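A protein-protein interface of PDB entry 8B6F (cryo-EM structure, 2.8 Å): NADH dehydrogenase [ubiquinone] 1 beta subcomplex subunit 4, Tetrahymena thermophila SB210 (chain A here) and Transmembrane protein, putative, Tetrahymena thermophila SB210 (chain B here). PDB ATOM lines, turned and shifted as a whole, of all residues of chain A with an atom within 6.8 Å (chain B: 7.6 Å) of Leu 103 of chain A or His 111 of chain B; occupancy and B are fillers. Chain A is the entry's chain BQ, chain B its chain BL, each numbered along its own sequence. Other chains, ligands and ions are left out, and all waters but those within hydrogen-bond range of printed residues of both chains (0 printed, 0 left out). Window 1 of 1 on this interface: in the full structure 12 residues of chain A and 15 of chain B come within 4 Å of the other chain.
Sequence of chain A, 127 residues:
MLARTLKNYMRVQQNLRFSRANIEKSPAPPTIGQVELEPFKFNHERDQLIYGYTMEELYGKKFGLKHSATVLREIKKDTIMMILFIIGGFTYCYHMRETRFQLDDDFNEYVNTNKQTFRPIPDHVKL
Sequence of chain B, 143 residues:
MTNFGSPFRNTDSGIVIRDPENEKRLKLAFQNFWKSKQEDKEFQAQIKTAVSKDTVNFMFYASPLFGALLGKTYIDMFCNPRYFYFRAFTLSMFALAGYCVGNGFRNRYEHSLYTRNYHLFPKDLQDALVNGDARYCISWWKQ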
ATOM      1  N   GLU A  98     -13.394  -2.178 -23.710  1.00  0.00           N
ATOM      2  CA  GLU A  98     -14.737  -2.713 -23.510  1.00  0.00           C
ATOM      3  C   GLU A  98     -15.499  -1.879 -22.491  1.00  0.00           C
ATOM      4  O   GLU A  98     -16.691  -1.606 -22.664  1.00  0.00           O
ATOM      5  CB  GLU A  98     -14.661  -4.173 -23.062  1.00  0.00           C
ATOM      6  CG  GLU A  98     -16.007  -4.794 -22.703  1.00  0.00           C
ATOM      7  CD  GLU A  98     -16.994  -4.764 -23.853  1.00  0.00           C
ATOM      8  OE1 GLU A  98     -16.555  -4.611 -25.011  1.00  0.00           O
ATOM      9  OE2 GLU A  98     -18.211  -4.891 -23.600  1.00  0.00           O
ATOM     10  N   THR A  99     -14.822  -1.465 -21.420  1.00  0.00           N
ATOM     11  CA  THR A  99     -15.455  -0.609 -20.425  1.00  0.00           C
ATOM     12  C   THR A  99     -15.907   0.706 -21.042  1.00  0.00           C
ATOM     13  O   THR A  99     -16.997   1.203 -20.735  1.00  0.00           O
ATOM     14  CB  THR A  99     -14.486  -0.359 -19.268  1.00  0.00           C
ATOM     15  OG1 THR A  99     -14.550  -1.447 -18.337  1.00  0.00           O
ATOM     16  CG2 THR A  99     -14.796   0.952 -18.560  1.00  0.00           C
ATOM     17  N   ARG A 100     -15.082   1.288 -21.911  1.00  0.00           N
ATOM     18  CA  ARG A 100     -15.469   2.519 -22.591  1.00  0.00           C
ATOM     19  C   ARG A 100     -16.708   2.301 -23.450  1.00  0.00           C
ATOM     20  O   ARG A 100     -17.602   3.154 -23.487  1.00  0.00           O
ATOM     21  CB  ARG A 100     -14.310   3.039 -23.437  1.00  0.00           C
ATOM     22  CG  ARG A 100     -14.548   4.428 -23.989  1.00  0.00           C
ATOM     23  CD  ARG A 100     -13.504   4.801 -25.020  1.00  0.00           C
ATOM     24  NE  ARG A 100     -13.720   4.129 -26.295  1.00  0.00           N
ATOM     25  CZ  ARG A 100     -14.712   4.406 -27.133  1.00  0.00           C
ATOM     26  NH1 ARG A 100     -15.634   5.307 -26.839  1.00  0.00           N
ATOM     27  NH2 ARG A 100     -14.783   3.760 -28.292  1.00  0.00           N
ATOM     28  N   PHE A 101     -16.776   1.171 -24.155  1.00  0.00           N
ATOM     29  CA  PHE A 101     -17.976   0.856 -24.921  1.00  0.00           C
ATOM     30  C   PHE A 101     -19.201   0.817 -24.017  1.00  0.00           C
ATOM     31  O   PHE A 101     -20.252   1.371 -24.358  1.00  0.00           O
ATOM     32  CB  PHE A 101     -17.814  -0.489 -25.634  1.00  0.00           C
ATOM     33  CG  PHE A 101     -16.741  -0.507 -26.687  1.00  0.00           C
ATOM     34  CD1 PHE A 101     -16.279   0.666 -27.266  1.00  0.00           C
ATOM     35  CD2 PHE A 101     -16.202  -1.710 -27.108  1.00  0.00           C
ATOM     36  CE1 PHE A 101     -15.298   0.633 -28.234  1.00  0.00           C
ATOM     37  CE2 PHE A 101     -15.222  -1.747 -28.075  1.00  0.00           C
ATOM     38  CZ  PHE A 101     -14.770  -0.575 -28.639  1.00  0.00           C
ATOM     39  N   GLN A 102     -19.084   0.173 -22.855  1.00  0.00           N
ATOM     40  CA  GLN A 102     -20.219   0.080 -21.941  1.00  0.00           C
ATOM     41  C   GLN A 102     -20.654   1.459 -21.462  1.00  0.00           C
ATOM     42  O   GLN A 102     -21.853   1.751 -21.393  1.00  0.00           O
ATOM     43  CB  GLN A 102     -19.861  -0.812 -20.754  1.00  0.00           C
ATOM     44  CG  GLN A 102     -19.559  -2.250 -21.142  1.00  0.00           C
ATOM     45  CD  GLN A 102     -19.008  -3.057 -19.987  1.00  0.00           C
ATOM     46  OE1 GLN A 102     -19.035  -2.617 -18.839  1.00  0.00           O
ATOM     47  NE2 GLN A 102     -18.497  -4.245 -20.288  1.00  0.00           N
ATOM     48  N   LEU A 103     -19.694   2.321 -21.122  1.00  0.00           N
ATOM     49  CA  LEU A 103     -20.036   3.672 -20.687  1.00  0.00           C
ATOM     50  C   LEU A 103     -20.738   4.442 -21.797  1.00  0.00           C
ATOM     51  O   LEU A 103     -21.704   5.171 -21.543  1.00  0.00           O
ATOM     52  CB  LEU A 103     -18.780   4.414 -20.234  1.00  0.00           C
ATOM     53  CG  LEU A 103     -18.082   3.866 -18.989  1.00  0.00           C
ATOM     54  CD1 LEU A 103     -16.788   4.615 -18.743  1.00  0.00           C
ATOM     55  CD2 LEU A 103     -18.987   3.953 -17.770  1.00  0.00           C
ATOM     56  N   ASP A 104     -20.260   4.304 -23.036  1.00  0.00           N
ATOM     57  CA  ASP A 104     -20.914   4.967 -24.157  1.00  0.00           C
ATOM     58  C   ASP A 104     -22.349   4.482 -24.318  1.00  0.00           C
ATOM     59  O   ASP A 104     -23.259   5.285 -24.554  1.00  0.00           O
ATOM     60  CB  ASP A 104     -20.125   4.732 -25.446  1.00  0.00           C
ATOM     61  CG  ASP A 104     -18.881   5.596 -25.537  1.00  0.00           C
ATOM     62  OD1 ASP A 104     -18.918   6.747 -25.057  1.00  0.00           O
ATOM     63  OD2 ASP A 104     -17.869   5.126 -26.096  1.00  0.00           O
ATOM     64  N   ASP A 105     -22.572   3.172 -24.193  1.00  0.00           N
ATOM     65  CA  ASP A 105     -23.931   2.647 -24.291  1.00  0.00           C
ATOM     66  C   ASP A 105     -24.822   3.227 -23.205  1.00  0.00           C
ATOM     67  O   ASP A 105     -25.964   3.619 -23.471  1.00  0.00           O
ATOM     68  CB  ASP A 105     -23.918   1.121 -24.192  1.00  0.00           C
ATOM     69  CG  ASP A 105     -23.451   0.452 -25.465  1.00  0.00           C
ATOM     70  OD1 ASP A 105     -23.790   0.952 -26.557  1.00  0.00           O
ATOM     71  OD2 ASP A 105     -22.748  -0.577 -25.377  1.00  0.00           O
ATOM     72  N   ASP A 106     -24.326   3.277 -21.968  1.00  0.00           N
ATOM     73  CA  ASP A 106     -25.124   3.816 -20.875  1.00  0.00           C
ATOM     74  C   ASP A 106     -25.497   5.270 -21.131  1.00  0.00           C
ATOM     75  O   ASP A 106     -26.654   5.668 -20.953  1.00  0.00           O
ATOM     76  CB  ASP A 106     -24.358   3.689 -19.560  1.00  0.00           C
ATOM     77  CG  ASP A 106     -23.989   2.257 -19.236  1.00  0.00           C
ATOM     78  OD1 ASP A 106     -24.436   1.348 -19.963  1.00  0.00           O
ATOM     79  OD2 ASP A 106     -23.247   2.042 -18.256  1.00  0.00           O
ATOM     80  N   PHE A 107     -24.527   6.081 -21.555  1.00  0.00           N
ATOM     81  CA  PHE A 107     -24.803   7.496 -21.773  1.00  0.00           C
ATOM     82  C   PHE A 107     -25.741   7.699 -22.954  1.00  0.00           C
ATOM     83  O   PHE A 107     -26.590   8.596 -22.933  1.00  0.00           O
ATOM     84  CB  PHE A 107     -23.503   8.268 -21.982  1.00  0.00           C
ATOM     85  CG  PHE A 107     -23.678   9.755 -21.920  1.00  0.00           C
ATOM     86  CD1 PHE A 107     -23.706  10.406 -20.699  1.00  0.00           C
ATOM     87  CD2 PHE A 107     -23.826  10.500 -23.077  1.00  0.00           C
ATOM     88  CE1 PHE A 107     -23.871  11.773 -20.633  1.00  0.00           C
ATOM     89  CE2 PHE A 107     -23.993  11.867 -23.016  1.00  0.00           C
ATOM     90  CZ  PHE A 107     -24.015  12.505 -21.793  1.00  0.00           C
ATOM     91  N   ASN A 108     -25.610   6.871 -23.993  1.00  0.00           N
ATOM     92  CA  ASN A 108     -26.533   6.961 -25.118  1.00  0.00           C
ATOM     93  C   ASN A 108     -27.955   6.658 -24.676  1.00  0.00           C
ATOM     94  O   ASN A 108     -28.900   7.341 -25.086  1.00  0.00           O
ATOM     95  CB  ASN A 108     -26.103   6.009 -26.235  1.00  0.00           C
ATOM     96  CG  ASN A 108     -24.808   6.431 -26.894  1.00  0.00           C
ATOM     97  OD1 ASN A 108     -24.454   7.609 -26.895  1.00  0.00           O
ATOM     98  ND2 ASN A 108     -24.093   5.469 -27.468  1.00  0.00           N
ATOM     99  N   PHE B   4     -13.764  12.534 -13.226  1.00  0.00           N
ATOM    100  CA  PHE B   4     -14.706  13.131 -14.161  1.00  0.00           C
ATOM    101  C   PHE B   4     -15.898  13.801 -13.499  1.00  0.00           C
ATOM    102  O   PHE B   4     -16.531  14.652 -14.130  1.00  0.00           O
ATOM    103  CB  PHE B   4     -15.229  12.067 -15.138  1.00  0.00           C
ATOM    104  CG  PHE B   4     -14.149  11.375 -15.916  1.00  0.00           C
ATOM    105  CD1 PHE B   4     -13.673  11.916 -17.099  1.00  0.00           C
ATOM    106  CD2 PHE B   4     -13.609  10.184 -15.465  1.00  0.00           C
ATOM    107  CE1 PHE B   4     -12.678  11.282 -17.817  1.00  0.00           C
ATOM    108  CE2 PHE B   4     -12.615   9.545 -16.180  1.00  0.00           C
ATOM    109  CZ  PHE B   4     -12.149  10.095 -17.356  1.00  0.00           C
ATOM    110  N   GLY B   5     -16.218  13.453 -12.260  1.00  0.00           N
ATOM    111  CA  GLY B   5     -17.403  13.998 -11.639  1.00  0.00           C
ATOM    112  C   GLY B   5     -18.656  13.345 -12.196  1.00  0.00           C
ATOM    113  O   GLY B   5     -18.624  12.305 -12.850  1.00  0.00           O
ATOM    114  N   SER B   6     -19.780  13.987 -11.916  1.00  0.00           N
ATOM    115  CA  SER B   6     -21.054  13.466 -12.380  1.00  0.00           C
ATOM    116  C   SER B   6     -21.127  13.554 -13.903  1.00  0.00           C
ATOM    117  O   SER B   6     -20.633  14.519 -14.494  1.00  0.00           O
ATOM    118  CB  SER B   6     -22.211  14.236 -11.751  1.00  0.00           C
ATOM    119  OG  SER B   6     -22.130  15.613 -12.066  1.00  0.00           O
ATOM    120  N   PRO B   7     -21.734  12.565 -14.567  1.00  0.00           N
ATOM    121  CA  PRO B   7     -21.851  12.636 -16.030  1.00  0.00           C
ATOM    122  C   PRO B   7     -22.935  13.579 -16.513  1.00  0.00           C
ATOM    123  O   PRO B   7     -22.886  14.003 -17.675  1.00  0.00           O
ATOM    124  CB  PRO B   7     -22.172  11.188 -16.420  1.00  0.00           C
ATOM    125  CG  PRO B   7     -22.915  10.663 -15.248  1.00  0.00           C
ATOM    126  CD  PRO B   7     -22.313  11.321 -14.032  1.00  0.00           C
ATOM    127  N   PHE B   8     -23.912  13.911 -15.671  1.00  0.00           N
ATOM    128  CA  PHE B   8     -25.027  14.740 -16.112  1.00  0.00           C
ATOM    129  C   PHE B   8     -24.636  16.208 -16.219  1.00  0.00           C
ATOM    130  O   PHE B   8     -25.105  16.911 -17.118  1.00  0.00           O
ATOM    131  CB  PHE B   8     -26.205  14.574 -15.153  1.00  0.00           C
ATOM    132  CG  PHE B   8     -26.528  13.144 -14.838  1.00  0.00           C
ATOM    133  CD1 PHE B   8     -27.250  12.371 -15.728  1.00  0.00           C
ATOM    134  CD2 PHE B   8     -26.111  12.574 -13.648  1.00  0.00           C
ATOM    135  CE1 PHE B   8     -27.548  11.055 -15.441  1.00  0.00           C
ATOM    136  CE2 PHE B   8     -26.405  11.259 -13.354  1.00  0.00           C
ATOM    137  CZ  PHE B   8     -27.125  10.499 -14.253  1.00  0.00           C
ATOM    138  N   THR B  49     -28.440  -3.410 -16.555  1.00  0.00           N
ATOM    139  CA  THR B  49     -27.120  -2.885 -16.244  1.00  0.00           C
ATOM    140  C   THR B  49     -26.092  -3.583 -17.125  1.00  0.00           C
ATOM    141  O   THR B  49     -26.284  -4.724 -17.548  1.00  0.00           O
ATOM    142  CB  THR B  49     -26.776  -3.070 -14.760  1.00  0.00           C
ATOM    143  OG1 THR B  49     -27.785  -2.451 -13.954  1.00  0.00           O
ATOM    144  CG2 THR B  49     -25.438  -2.432 -14.434  1.00  0.00           C
ATOM    145  N   ALA B  50     -24.995  -2.874 -17.395  1.00  0.00           N
ATOM    146  CA  ALA B  50     -23.946  -3.410 -18.255  1.00  0.00           C
ATOM    147  C   ALA B  50     -23.312  -4.649 -17.643  1.00  0.00           C
ATOM    148  O   ALA B  50     -23.044  -5.632 -18.345  1.00  0.00           O
ATOM    149  CB  ALA B  50     -22.888  -2.337 -18.509  1.00  0.00           C
ATOM    150  N   GLY B 104     -13.215   0.877  -9.354  1.00  0.00           N
ATOM    151  CA  GLY B 104     -13.677   1.316 -10.658  1.00  0.00           C
ATOM    152  C   GLY B 104     -14.813   0.465 -11.190  1.00  0.00           C
ATOM    153  O   GLY B 104     -15.770   0.982 -11.768  1.00  0.00           O
ATOM    154  N   PHE B 105     -14.721  -0.853 -11.009  1.00  0.00           N
ATOM    155  CA  PHE B 105     -15.828  -1.726 -11.385  1.00  0.00           C
ATOM    156  C   PHE B 105     -17.109  -1.307 -10.674  1.00  0.00           C
ATOM    157  O   PHE B 105     -18.168  -1.177 -11.296  1.00  0.00           O
ATOM    158  CB  PHE B 105     -15.486  -3.179 -11.053  1.00  0.00           C
ATOM    159  CG  PHE B 105     -15.190  -4.019 -12.257  1.00  0.00           C
ATOM    160  CD1 PHE B 105     -16.205  -4.679 -12.924  1.00  0.00           C
ATOM    161  CD2 PHE B 105     -13.892  -4.156 -12.717  1.00  0.00           C
ATOM    162  CE1 PHE B 105     -15.934  -5.455 -14.030  1.00  0.00           C
ATOM    163  CE2 PHE B 105     -13.613  -4.931 -13.822  1.00  0.00           C
ATOM    164  CZ  PHE B 105     -14.636  -5.582 -14.480  1.00  0.00           C
ATOM    165  N   ARG B 106     -17.027  -1.103  -9.358  1.00  0.00           N
ATOM    166  CA  ARG B 106     -18.212  -0.743  -8.586  1.00  0.00           C
ATOM    167  C   ARG B 106     -18.772   0.603  -9.027  1.00  0.00           C
ATOM    168  O   ARG B 106     -19.991   0.765  -9.159  1.00  0.00           O
ATOM    169  CB  ARG B 106     -17.872  -0.725  -7.096  1.00  0.00           C
ATOM    170  CG  ARG B 106     -19.050  -0.393  -6.199  1.00  0.00           C
ATOM    171  CD  ARG B 106     -18.715  -0.656  -4.741  1.00  0.00           C
ATOM    172  NE  ARG B 106     -17.491   0.022  -4.332  1.00  0.00           N
ATOM    173  CZ  ARG B 106     -17.432   1.269  -3.882  1.00  0.00           C
ATOM    174  NH1 ARG B 106     -18.518   2.017  -3.773  1.00  0.00           N
ATOM    175  NH2 ARG B 106     -16.254   1.778  -3.533  1.00  0.00           N
ATOM    176  N   ASN B 107     -17.897   1.586  -9.248  1.00  0.00           N
ATOM    177  CA  ASN B 107     -18.355   2.915  -9.638  1.00  0.00           C
ATOM    178  C   ASN B 107     -18.983   2.903 -11.024  1.00  0.00           C
ATOM    179  O   ASN B 107     -19.975   3.599 -11.267  1.00  0.00           O
ATOM    180  CB  ASN B 107     -17.195   3.904  -9.591  1.00  0.00           C
ATOM    181  CG  ASN B 107     -17.665   5.341  -9.563  1.00  0.00           C
ATOM    182  OD1 ASN B 107     -18.735   5.663 -10.075  1.00  0.00           O
ATOM    183  ND2 ASN B 107     -16.870   6.211  -8.958  1.00  0.00           N
ATOM    184  N   ARG B 108     -18.415   2.131 -11.950  1.00  0.00           N
ATOM    185  CA  ARG B 108     -19.024   2.002 -13.268  1.00  0.00           C
ATOM    186  C   ARG B 108     -20.362   1.285 -13.200  1.00  0.00           C
ATOM    187  O   ARG B 108     -21.272   1.603 -13.974  1.00  0.00           O
ATOM    188  CB  ARG B 108     -18.073   1.280 -14.219  1.00  0.00           C
ATOM    189  CG  ARG B 108     -16.860   2.113 -14.583  1.00  0.00           C
ATOM    190  CD  ARG B 108     -16.032   1.452 -15.661  1.00  0.00           C
ATOM    191  NE  ARG B 108     -15.295   0.289 -15.177  1.00  0.00           N
ATOM    192  CZ  ARG B 108     -15.744  -0.960 -15.205  1.00  0.00           C
ATOM    193  NH1 ARG B 108     -16.945  -1.257 -15.676  1.00  0.00           N
ATOM    194  NH2 ARG B 108     -14.966  -1.937 -14.749  1.00  0.00           N
ATOM    195  N   TYR B 109     -20.507   0.310 -12.302  1.00  0.00           N
ATOM    196  CA  TYR B 109     -21.816  -0.297 -12.100  1.00  0.00           C
ATOM    197  C   TYR B 109     -22.827   0.738 -11.628  1.00  0.00           C
ATOM    198  O   TYR B 109     -23.966   0.766 -12.104  1.00  0.00           O
ATOM    199  CB  TYR B 109     -21.716  -1.430 -11.080  1.00  0.00           C
ATOM    200  CG  TYR B 109     -23.057  -2.002 -10.683  1.00  0.00           C
ATOM    201  CD1 TYR B 109     -23.640  -3.026 -11.415  1.00  0.00           C
ATOM    202  CD2 TYR B 109     -23.747  -1.508  -9.585  1.00  0.00           C
ATOM    203  CE1 TYR B 109     -24.870  -3.548 -11.060  1.00  0.00           C
ATOM    204  CE2 TYR B 109     -24.976  -2.023  -9.221  1.00  0.00           C
ATOM    205  CZ  TYR B 109     -25.532  -3.041  -9.964  1.00  0.00           C
ATOM    206  OH  TYR B 109     -26.756  -3.558  -9.606  1.00  0.00           O
ATOM    207  N   GLU B 110     -22.430   1.595 -10.687  1.00  0.00           N
ATOM    208  CA  GLU B 110     -23.336   2.634 -10.214  1.00  0.00           C
ATOM    209  C   GLU B 110     -23.697   3.593 -11.340  1.00  0.00           C
ATOM    210  O   GLU B 110     -24.861   3.981 -11.490  1.00  0.00           O
ATOM    211  CB  GLU B 110     -22.701   3.386  -9.045  1.00  0.00           C
ATOM    212  CG  GLU B 110     -23.600   4.443  -8.432  1.00  0.00           C
ATOM    213  CD  GLU B 110     -22.969   5.106  -7.225  1.00  0.00           C
ATOM    214  OE1 GLU B 110     -21.844   4.713  -6.852  1.00  0.00           O
ATOM    215  OE2 GLU B 110     -23.597   6.018  -6.646  1.00  0.00           O
ATOM    216  N   HIS B 111     -22.708   3.984 -12.145  1.00  0.00           N
ATOM    217  CA  HIS B 111     -22.969   4.866 -13.277  1.00  0.00           C
ATOM    218  C   HIS B 111     -23.967   4.238 -14.235  1.00  0.00           C
ATOM    219  O   HIS B 111     -24.914   4.890 -14.687  1.00  0.00           O
ATOM    220  CB  HIS B 111     -21.655   5.176 -13.995  1.00  0.00           C
ATOM    221  CG  HIS B 111     -21.826   5.927 -15.278  1.00  0.00           C
ATOM    222  ND1 HIS B 111     -22.149   5.306 -16.466  1.00  0.00           N
ATOM    223  CD2 HIS B 111     -21.708   7.245 -15.564  1.00  0.00           C
ATOM    224  CE1 HIS B 111     -22.226   6.208 -17.426  1.00  0.00           C
ATOM    225  NE2 HIS B 111     -21.962   7.393 -16.907  1.00  0.00           N
ATOM    226  N   SER B 112     -23.766   2.963 -14.559  1.00  0.00           N
ATOM    227  CA  SER B 112     -24.693   2.258 -15.433  1.00  0.00           C
ATOM    228  C   SER B 112     -26.082   2.172 -14.814  1.00  0.00           C
ATOM    229  O   SER B 112     -27.091   2.348 -15.506  1.00  0.00           O
ATOM    230  CB  SER B 112     -24.158   0.867 -15.749  1.00  0.00           C
ATOM    231  OG  SER B 112     -25.010   0.224 -16.671  1.00  0.00           O
ATOM    232  N   LEU B 113     -26.152   1.896 -13.512  1.00  0.00           N
ATOM    233  CA  LEU B 113     -27.445   1.772 -12.850  1.00  0.00           C
ATOM    234  C   LEU B 113     -28.248   3.060 -12.948  1.00  0.00           C
ATOM    235  O   LEU B 113     -29.456   3.027 -13.208  1.00  0.00           O
ATOM    236  CB  LEU B 113     -27.243   1.387 -11.382  1.00  0.00           C
ATOM    237  CG  LEU B 113     -28.509   1.211 -10.539  1.00  0.00           C
ATOM    238  CD1 LEU B 113     -29.232  -0.072 -10.911  1.00  0.00           C
ATOM    239  CD2 LEU B 113     -28.176   1.227  -9.060  1.00  0.00           C
ATOM    240  N   TYR B 114     -27.605   4.204 -12.739  1.00  0.00           N
ATOM    241  CA  TYR B 114     -28.306   5.480 -12.741  1.00  0.00           C
ATOM    242  C   TYR B 114     -28.402   6.119 -14.120  1.00  0.00           C
ATOM    243  O   TYR B 114     -29.052   7.159 -14.255  1.00  0.00           O
ATOM    244  CB  TYR B 114     -27.619   6.446 -11.773  1.00  0.00           C
ATOM    245  CG  TYR B 114     -27.977   6.181 -10.333  1.00  0.00           C
ATOM    246  CD1 TYR B 114     -29.120   6.727  -9.770  1.00  0.00           C
ATOM    247  CD2 TYR B 114     -27.181   5.365  -9.542  1.00  0.00           C
ATOM    248  CE1 TYR B 114     -29.456   6.477  -8.457  1.00  0.00           C
ATOM    249  CE2 TYR B 114     -27.508   5.109  -8.227  1.00  0.00           C
ATOM    250  CZ  TYR B 114     -28.647   5.668  -7.690  1.00  0.00           C
ATOM    251  OH  TYR B 114     -28.972   5.414  -6.379  1.00  0.00           O
ATOM    252  N   THR B 115     -27.775   5.536 -15.142  1.00  0.00           N
ATOM    253  CA  THR B 115     -27.907   6.033 -16.507  1.00  0.00           C
ATOM    254  C   THR B 115     -28.857   5.191 -17.350  1.00  0.00           C
ATOM    255  O   THR B 115     -29.799   5.730 -17.937  1.00  0.00           O
ATOM    256  CB  THR B 115     -26.528   6.092 -17.177  1.00  0.00           C
ATOM    257  OG1 THR B 115     -25.754   4.950 -16.788  1.00  0.00           O
ATOM    258  CG2 THR B 115     -25.790   7.363 -16.786  1.00  0.00           C
ATOM    259  N   ARG B 116     -28.634   3.876 -17.424  1.00  0.00           N
ATOM    260  CA  ARG B 116     -29.486   3.040 -18.266  1.00  0.00           C
ATOM    261  C   ARG B 116     -30.933   3.059 -17.796  1.00  0.00           C
ATOM    262  O   ARG B 116     -31.852   2.942 -18.614  1.00  0.00           O
ATOM    263  CB  ARG B 116     -28.965   1.604 -18.292  1.00  0.00           C
ATOM    264  CG  ARG B 116     -27.675   1.415 -19.072  1.00  0.00           C
ATOM    265  CD  ARG B 116     -27.211  -0.033 -19.006  1.00  0.00           C
ATOM    266  NE  ARG B 116     -26.020  -0.273 -19.814  1.00  0.00           N
ATOM    267  CZ  ARG B 116     -26.031  -0.706 -21.069  1.00  0.00           C
ATOM    268  NH1 ARG B 116     -27.163  -0.951 -21.708  1.00  0.00           N
ATOM    269  NH2 ARG B 116     -24.876  -0.892 -21.700  1.00  0.00           N
ATOM    270  N   ASN B 117     -31.156   3.200 -16.490  1.00  0.00           N
ATOM    271  CA  ASN B 117     -32.494   3.200 -15.916  1.00  0.00           C
ATOM    272  C   ASN B 117     -33.031   4.609 -15.706  1.00  0.00           C
ATOM    273  O   ASN B 117     -33.929   4.810 -14.883  1.00  0.00           O
ATOM    274  CB  ASN B 117     -32.494   2.433 -14.594  1.00  0.00           C
ATOM    275  CG  ASN B 117     -31.817   1.087 -14.707  1.00  0.00           C
ATOM    276  OD1 ASN B 117     -31.873   0.437 -15.750  1.00  0.00           O
ATOM    277  ND2 ASN B 117     -31.166   0.661 -13.635  1.00  0.00           N
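OD2 of Asp 106 of chain A lies close to OG of Ser 112 of chain B (3.0 Å).
The side-chain carboxylate of Asp 106 of chain A lies within salt-bridge range of the guanidinium group of Arg 116 of chain B (2.9 Å).
Printed residues of chain B within 4 Å of Thr 99 of chain A: Arg 108 (3.2 Å).
Of chain B, only His 111 (3.7 Å) comes within 4 Å of Leu 103 of chain A.
Printed residues of chain B within 4 Å of Phe 107 of chain A: Pro 7 (3.8 Å).
Printed residues of chain A within 4 Å of Pro 7 of chain B: Phe 107 (3.8 Å).
His 111 of chain B touches just these residues of chain A: Leu 103 and Asp 106.
Printed residues of chain A within 4 Å of Ser 112 of chain B: Asp 106 (2.9 Å).
The nearest residue of chain A that does not touch His 111 of chain B is Phe 107 of chain A (4.7 Å).
OG of Ser 112 of chain B lies within hydrogen-bond range of N of Ala 50 of chain B (3.2 Å).
O of Ser 112 of chain B sits at hydrogen-bond distance from OG1 of Thr 115 of chain B, at 3.2 Å.
OG of Ser 112 of chain B lies close to NE of Arg 116 of chain B (3.3 Å).
OE2 of Glu 98 of chain A sits at hydrogen-bond distance from NE2 of Gln 102 of chain A (3.4 Å).
Among the printed residues, merely in contact across the chains: Thr 99 of chain A with Arg 108 of chain B (3.2 Å), Gln 102 of chain A with Ala 50 of chain B (3.9 Å), Leu 103 of chain A with His 111 of chain B (3.7 Å), Asp 105 of chain A with Arg 116 of chain B (3.3 Å), Asp 106 of chain A with His 111 of chain B (3.9 Å), Asp 106 of chain A with Thr 115 of chain B (3.4 Å) and Phe 107 of chain A with Pro 7 of chain B (3.8 Å).
Hydrophobic or aromatic side chains of chain B that line the printed part of chain A: Ala 50 and His 111.
Of the 11 printed residues of chain A, 6 touch a printed residue of chain B.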
